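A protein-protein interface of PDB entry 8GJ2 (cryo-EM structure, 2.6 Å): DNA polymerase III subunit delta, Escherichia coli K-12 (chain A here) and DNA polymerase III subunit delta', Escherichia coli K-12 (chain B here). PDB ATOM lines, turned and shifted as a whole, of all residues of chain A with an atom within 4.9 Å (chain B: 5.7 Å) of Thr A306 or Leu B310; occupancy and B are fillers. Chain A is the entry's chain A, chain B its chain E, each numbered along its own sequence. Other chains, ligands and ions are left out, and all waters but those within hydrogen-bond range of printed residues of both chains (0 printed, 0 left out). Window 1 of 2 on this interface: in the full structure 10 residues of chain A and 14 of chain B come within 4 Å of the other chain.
NE2 of Gln A251 sits at hydrogen-bond distance from OD1 of Asn B307 (2.9 Å). The side-chain hydroxyl (OG1) of Thr A306 sits close to the side-chain carboxylate (OD2) of Asp B314 (3.4 Å). The side-chain carboxylate of Glu A309 lies close to the backbone NH of Asn B307 (3.2 Å).
OG1 of Thr A306 is in hydrogen-bond range of O of Val A302 (2.9 Å). The backbone NH (N) of Glu B309 sits at hydrogen-bond distance from the side-chain amide oxygen (OD1) of Asn B307 (3.4 Å). The backbone NH (N) of Leu B310 sits at hydrogen-bond distance from the side-chain amide oxygen (OD1) of Asn B307 (3.1 Å). O of Glu B309 sits at hydrogen-bond distance from OG1 of Thr B313 (2.9 Å).
Gln A251 touches Leu B310. Glu B309 touches Leu A255 (OE2 to CD1, 3.9 Å). OG1 of Thr A306 touches CG of Leu B310, 3.4 Å away. CG2 of Thr A306 touches CD1 of Leu B311, 3.9 Å away. OE1 of Glu A309 touches CD2 of Leu B310 (3.4 Å). Leu B311 touches Glu A309.
Thr A306 touches just these residues of chain B: Leu B310 (3.4 Å), Leu B311 (3.9 Å) and Asp B314 (3.4 Å). Of chain A, only Gln A251 (3.7 Å), Thr A306 (3.4 Å) and Glu A309 (3.4 Å) come within 4 Å of Leu B310. Of the printed residues of chain B, Gln A251 touches Asn B307 (2.9 Å) and Leu B310 (3.7 Å). Printed residues of chain A within 4 Å of Asn B307: Gln A251 and Glu A309. Of the printed residues of chain B, Glu A309 touches Asn B307 (3.1 Å), Leu B310 (3.4 Å) and Leu B311 (3.7 Å). Printed residues of chain A within 4 Å of Leu B311: Thr A306 (3.9 Å) and Glu A309 (3.7 Å). Leu A310 touches none of the printed residues of chain B. Leu B315 touches none of the printed residues of chain A. The nearest printed residue of chain A that does not touch Asn B307 is Leu A255 (5.9 Å).
Of the 9 printed residues of chain B, 5 touch a printed residue of chain A. Printed residues of chain B that touch a printed residue of chain A: Asn B307, Glu B309, Leu B310, Leu B311 and Asp B314. Hydrophobic or aromatic side chains of chain B within 4 Å of the printed part of chain A: Leu B310 and Leu B311. Along chain B the printed residues that touch a printed residue of chain A span positions 307 to 314. Printed residues of chain A that touch a printed residue of chain B: Gln A251, Leu A255, Thr A306 and Glu A309. Among the printed residues, 9 pairs touch across the chains.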
ATOM      1  N   GLN A 251      -7.930  -2.167  14.474  1.00  0.00           N
ATOM      2  CA  GLN A 251      -7.291  -2.611  15.707  1.00  0.00           C
ATOM      3  C   GLN A 251      -5.795  -2.790  15.519  1.00  0.00           C
ATOM      4  O   GLN A 251      -5.004  -2.410  16.389  1.00  0.00           O
ATOM      5  CB  GLN A 251      -7.928  -3.920  16.177  1.00  0.00           C
ATOM      6  CG  GLN A 251      -7.270  -4.549  17.399  1.00  0.00           C
ATOM      7  CD  GLN A 251      -7.877  -5.888  17.757  1.00  0.00           C
ATOM      8  OE1 GLN A 251      -8.983  -6.218  17.327  1.00  0.00           O
ATOM      9  NE2 GLN A 251      -7.151  -6.674  18.542  1.00  0.00           N
ATOM     10  N   LEU A 255      -3.299  -0.552  17.820  1.00  0.00           N
ATOM     11  CA  LEU A 255      -2.375  -1.141  18.783  1.00  0.00           C
ATOM     12  C   LEU A 255      -0.931  -0.801  18.435  1.00  0.00           C
ATOM     13  O   LEU A 255      -0.120  -0.520  19.329  1.00  0.00           O
ATOM     14  CB  LEU A 255      -2.574  -2.655  18.844  1.00  0.00           C
ATOM     15  CG  LEU A 255      -3.935  -3.133  19.358  1.00  0.00           C
ATOM     16  CD1 LEU A 255      -4.026  -4.649  19.296  1.00  0.00           C
ATOM     17  CD2 LEU A 255      -4.195  -2.642  20.775  1.00  0.00           C
ATOM     18  N   VAL A 302      -9.294   3.071  22.262  1.00  0.00           N
ATOM     19  CA  VAL A 302      -9.239   1.640  22.550  1.00  0.00           C
ATOM     20  C   VAL A 302     -10.463   1.212  23.349  1.00  0.00           C
ATOM     21  O   VAL A 302     -11.047   0.150  23.097  1.00  0.00           O
ATOM     22  CB  VAL A 302      -7.932   1.293  23.286  1.00  0.00           C
ATOM     23  CG1 VAL A 302      -7.978  -0.133  23.810  1.00  0.00           C
ATOM     24  CG2 VAL A 302      -6.740   1.479  22.362  1.00  0.00           C
ATOM     25  N   GLN A 303     -10.862   2.021  24.333  1.00  0.00           N
ATOM     26  CA  GLN A 303     -12.048   1.699  25.118  1.00  0.00           C
ATOM     27  C   GLN A 303     -13.290   1.641  24.236  1.00  0.00           C
ATOM     28  O   GLN A 303     -14.105   0.718  24.356  1.00  0.00           O
ATOM     29  CB  GLN A 303     -12.226   2.734  26.229  1.00  0.00           C
ATOM     30  CG  GLN A 303     -13.424   2.497  27.132  1.00  0.00           C
ATOM     31  CD  GLN A 303     -13.543   3.544  28.221  1.00  0.00           C
ATOM     32  OE1 GLN A 303     -12.690   4.423  28.345  1.00  0.00           O
ATOM     33  NE2 GLN A 303     -14.603   3.458  29.013  1.00  0.00           N
ATOM     34  N   LEU A 304     -13.449   2.618  23.342  1.00  0.00           N
ATOM     35  CA  LEU A 304     -14.605   2.630  22.453  1.00  0.00           C
ATOM     36  C   LEU A 304     -14.582   1.435  21.510  1.00  0.00           C
ATOM     37  O   LEU A 304     -15.626   0.829  21.241  1.00  0.00           O
ATOM     38  CB  LEU A 304     -14.642   3.941  21.667  1.00  0.00           C
ATOM     39  CG  LEU A 304     -15.824   4.148  20.718  1.00  0.00           C
ATOM     40  CD1 LEU A 304     -17.147   4.045  21.459  1.00  0.00           C
ATOM     41  CD2 LEU A 304     -15.708   5.493  20.023  1.00  0.00           C
ATOM     42  N   LEU A 305     -13.403   1.080  20.995  1.00  0.00           N
ATOM     43  CA  LEU A 305     -13.299  -0.077  20.113  1.00  0.00           C
ATOM     44  C   LEU A 305     -13.673  -1.360  20.845  1.00  0.00           C
ATOM     45  O   LEU A 305     -14.388  -2.210  20.301  1.00  0.00           O
ATOM     46  CB  LEU A 305     -11.881  -0.171  19.550  1.00  0.00           C
ATOM     47  CG  LEU A 305     -11.606  -1.280  18.533  1.00  0.00           C
ATOM     48  CD1 LEU A 305     -12.462  -1.103  17.292  1.00  0.00           C
ATOM     49  CD2 LEU A 305     -10.133  -1.304  18.165  1.00  0.00           C
ATOM     50  N   THR A 306     -13.198  -1.520  22.083  1.00  0.00           N
ATOM     51  CA  THR A 306     -13.543  -2.707  22.859  1.00  0.00           C
ATOM     52  C   THR A 306     -15.039  -2.760  23.143  1.00  0.00           C
ATOM     53  O   THR A 306     -15.659  -3.828  23.058  1.00  0.00           O
ATOM     54  CB  THR A 306     -12.752  -2.729  24.166  1.00  0.00           C
ATOM     55  OG1 THR A 306     -11.351  -2.639  23.881  1.00  0.00           O
ATOM     56  CG2 THR A 306     -13.025  -4.011  24.938  1.00  0.00           C
ATOM     57  N   ARG A 307     -15.635  -1.618  23.490  1.00  0.00           N
ATOM     58  CA  ARG A 307     -17.072  -1.584  23.739  1.00  0.00           C
ATOM     59  C   ARG A 307     -17.851  -1.952  22.482  1.00  0.00           C
ATOM     60  O   ARG A 307     -18.833  -2.702  22.546  1.00  0.00           O
ATOM     61  CB  ARG A 307     -17.481  -0.198  24.236  1.00  0.00           C
ATOM     62  CG  ARG A 307     -18.785  -0.174  25.010  1.00  0.00           C
ATOM     63  CD  ARG A 307     -19.249   1.251  25.248  1.00  0.00           C
ATOM     64  NE  ARG A 307     -19.791   1.854  24.036  1.00  0.00           N
ATOM     65  CZ  ARG A 307     -20.032   3.149  23.881  1.00  0.00           C
ATOM     66  NH1 ARG A 307     -19.762   4.024  24.836  1.00  0.00           N
ATOM     67  NH2 ARG A 307     -20.553   3.578  22.735  1.00  0.00           N
ATOM     68  N   THR A 308     -17.426  -1.431  21.329  1.00  0.00           N
ATOM     69  CA  THR A 308     -18.086  -1.766  20.072  1.00  0.00           C
ATOM     70  C   THR A 308     -17.968  -3.254  19.773  1.00  0.00           C
ATOM     71  O   THR A 308     -18.936  -3.884  19.331  1.00  0.00           O
ATOM     72  CB  THR A 308     -17.485  -0.946  18.930  1.00  0.00           C
ATOM     73  OG1 THR A 308     -17.488   0.443  19.281  1.00  0.00           O
ATOM     74  CG2 THR A 308     -18.281  -1.143  17.651  1.00  0.00           C
ATOM     75  N   GLU A 309     -16.787  -3.831  19.999  1.00  0.00           N
ATOM     76  CA  GLU A 309     -16.613  -5.259  19.761  1.00  0.00           C
ATOM     77  C   GLU A 309     -17.526  -6.077  20.664  1.00  0.00           C
ATOM     78  O   GLU A 309     -18.164  -7.033  20.211  1.00  0.00           O
ATOM     79  CB  GLU A 309     -15.155  -5.660  19.981  1.00  0.00           C
ATOM     80  CG  GLU A 309     -14.835  -7.082  19.534  1.00  0.00           C
ATOM     81  CD  GLU A 309     -13.520  -7.595  20.088  1.00  0.00           C
ATOM     82  OE1 GLU A 309     -13.080  -7.098  21.145  1.00  0.00           O
ATOM     83  OE2 GLU A 309     -12.928  -8.499  19.464  1.00  0.00           O
ATOM     84  N   LEU A 310     -17.598  -5.720  21.948  1.00  0.00           N
ATOM     85  CA  LEU A 310     -18.469  -6.455  22.859  1.00  0.00           C
ATOM     86  C   LEU A 310     -19.926  -6.343  22.431  1.00  0.00           C
ATOM     87  O   LEU A 310     -20.658  -7.340  22.422  1.00  0.00           O
ATOM     88  CB  LEU A 310     -18.290  -5.944  24.289  1.00  0.00           C
ATOM     89  CG  LEU A 310     -16.988  -6.336  24.990  1.00  0.00           C
ATOM     90  CD1 LEU A 310     -16.840  -5.576  26.296  1.00  0.00           C
ATOM     91  CD2 LEU A 310     -16.938  -7.836  25.240  1.00  0.00           C
ATOM     92  N   ASN B 307     -11.834 -11.088  21.088  1.00  0.00           N
ATOM     93  CA  ASN B 307     -10.409 -10.917  20.836  1.00  0.00           C
ATOM     94  C   ASN B 307      -9.680 -10.766  22.165  1.00  0.00           C
ATOM     95  O   ASN B 307      -9.996  -9.872  22.957  1.00  0.00           O
ATOM     96  CB  ASN B 307     -10.164  -9.703  19.940  1.00  0.00           C
ATOM     97  CG  ASN B 307      -8.747  -9.652  19.407  1.00  0.00           C
ATOM     98  OD1 ASN B 307      -7.867  -9.038  20.008  1.00  0.00           O
ATOM     99  ND2 ASN B 307      -8.520 -10.300  18.270  1.00  0.00           N
ATOM    100  N   ARG B 308      -8.701 -11.641  22.404  1.00  0.00           N
ATOM    101  CA  ARG B 308      -8.015 -11.665  23.692  1.00  0.00           C
ATOM    102  C   ARG B 308      -7.120 -10.442  23.872  1.00  0.00           C
ATOM    103  O   ARG B 308      -7.143  -9.789  24.924  1.00  0.00           O
ATOM    104  CB  ARG B 308      -7.194 -12.950  23.805  1.00  0.00           C
ATOM    105  CG  ARG B 308      -6.594 -13.201  25.173  1.00  0.00           C
ATOM    106  CD  ARG B 308      -5.576 -14.333  25.138  1.00  0.00           C
ATOM    107  NE  ARG B 308      -6.097 -15.534  24.495  1.00  0.00           N
ATOM    108  CZ  ARG B 308      -5.907 -15.862  23.222  1.00  0.00           C
ATOM    109  NH1 ARG B 308      -5.204 -15.096  22.402  1.00  0.00           N
ATOM    110  NH2 ARG B 308      -6.435 -16.991  22.760  1.00  0.00           N
ATOM    111  N   GLU B 309      -6.321 -10.120  22.851  1.00  0.00           N
ATOM    112  CA  GLU B 309      -5.326  -9.062  22.992  1.00  0.00           C
ATOM    113  C   GLU B 309      -5.983  -7.715  23.260  1.00  0.00           C
ATOM    114  O   GLU B 309      -5.514  -6.947  24.108  1.00  0.00           O
ATOM    115  CB  GLU B 309      -4.459  -8.993  21.736  1.00  0.00           C
ATOM    116  CG  GLU B 309      -3.311  -7.998  21.826  1.00  0.00           C
ATOM    117  CD  GLU B 309      -2.470  -7.964  20.566  1.00  0.00           C
ATOM    118  OE1 GLU B 309      -2.825  -8.662  19.594  1.00  0.00           O
ATOM    119  OE2 GLU B 309      -1.453  -7.239  20.549  1.00  0.00           O
ATOM    120  N   LEU B 310      -7.064  -7.406  22.541  1.00  0.00           N
ATOM    121  CA  LEU B 310      -7.732  -6.124  22.730  1.00  0.00           C
ATOM    122  C   LEU B 310      -8.276  -5.998  24.148  1.00  0.00           C
ATOM    123  O   LEU B 310      -8.113  -4.960  24.800  1.00  0.00           O
ATOM    124  CB  LEU B 310      -8.854  -5.968  21.702  1.00  0.00           C
ATOM    125  CG  LEU B 310      -9.592  -4.627  21.685  1.00  0.00           C
ATOM    126  CD1 LEU B 310      -8.645  -3.485  21.356  1.00  0.00           C
ATOM    127  CD2 LEU B 310     -10.739  -4.670  20.694  1.00  0.00           C
ATOM    128  N   LEU B 311      -8.920  -7.057  24.646  1.00  0.00           N
ATOM    129  CA  LEU B 311      -9.470  -7.014  25.997  1.00  0.00           C
ATOM    130  C   LEU B 311      -8.370  -6.850  27.038  1.00  0.00           C
ATOM    131  O   LEU B 311      -8.508  -6.054  27.973  1.00  0.00           O
ATOM    132  CB  LEU B 311     -10.283  -8.277  26.277  1.00  0.00           C
ATOM    133  CG  LEU B 311     -11.793  -8.155  26.058  1.00  0.00           C
ATOM    134  CD1 LEU B 311     -12.109  -7.803  24.613  1.00  0.00           C
ATOM    135  CD2 LEU B 311     -12.493  -9.440  26.466  1.00  0.00           C
ATOM    136  N   ILE B 312      -7.271  -7.595  26.897  1.00  0.00           N
ATOM    137  CA  ILE B 312      -6.201  -7.495  27.886  1.00  0.00           C
ATOM    138  C   ILE B 312      -5.567  -6.109  27.852  1.00  0.00           C
ATOM    139  O   ILE B 312      -5.268  -5.522  28.901  1.00  0.00           O
ATOM    140  CB  ILE B 312      -5.161  -8.609  27.668  1.00  0.00           C
ATOM    141  CG1 ILE B 312      -5.804  -9.976  27.925  1.00  0.00           C
ATOM    142  CG2 ILE B 312      -3.955  -8.397  28.585  1.00  0.00           C
ATOM    143  CD1 ILE B 312      -4.913 -11.160  27.618  1.00  0.00           C
ATOM    144  N   THR B 313      -5.343  -5.563  26.654  1.00  0.00           N
ATOM    145  CA  THR B 313      -4.768  -4.226  26.552  1.00  0.00           C
ATOM    146  C   THR B 313      -5.687  -3.186  27.177  1.00  0.00           C
ATOM    147  O   THR B 313      -5.228  -2.290  27.900  1.00  0.00           O
ATOM    148  CB  THR B 313      -4.494  -3.884  25.087  1.00  0.00           C
ATOM    149  OG1 THR B 313      -3.569  -4.829  24.537  1.00  0.00           O
ATOM    150  CG2 THR B 313      -3.920  -2.481  24.962  1.00  0.00           C
ATOM    151  N   ASP B 314      -6.992  -3.288  26.910  1.00  0.00           N
ATOM    152  CA  ASP B 314      -7.938  -2.356  27.510  1.00  0.00           C
ATOM    153  C   ASP B 314      -7.922  -2.469  29.028  1.00  0.00           C
ATOM    154  O   ASP B 314      -7.951  -1.455  29.733  1.00  0.00           O
ATOM    155  CB  ASP B 314      -9.342  -2.615  26.966  1.00  0.00           C
ATOM    156  CG  ASP B 314     -10.344  -1.571  27.415  1.00  0.00           C
ATOM    157  OD1 ASP B 314      -9.927  -0.566  28.029  1.00  0.00           O
ATOM    158  OD2 ASP B 314     -11.552  -1.753  27.155  1.00  0.00           O
ATOM    159  N   LEU B 315      -7.870  -3.696  29.549  1.00  0.00           N
ATOM    160  CA  LEU B 315      -7.831  -3.886  30.996  1.00  0.00           C
ATOM    161  C   LEU B 315      -6.589  -3.243  31.600  1.00  0.00           C
ATOM    162  O   LEU B 315      -6.666  -2.562  32.630  1.00  0.00           O
ATOM    163  CB  LEU B 315      -7.877  -5.381  31.323  1.00  0.00           C
ATOM    164  CG  LEU B 315      -7.647  -5.780  32.784  1.00  0.00           C
ATOM    165  CD1 LEU B 315      -8.677  -5.130  33.693  1.00  0.00           C
ATOM    166  CD2 LEU B 315      -7.674  -7.291  32.930  1.00  0.00           C
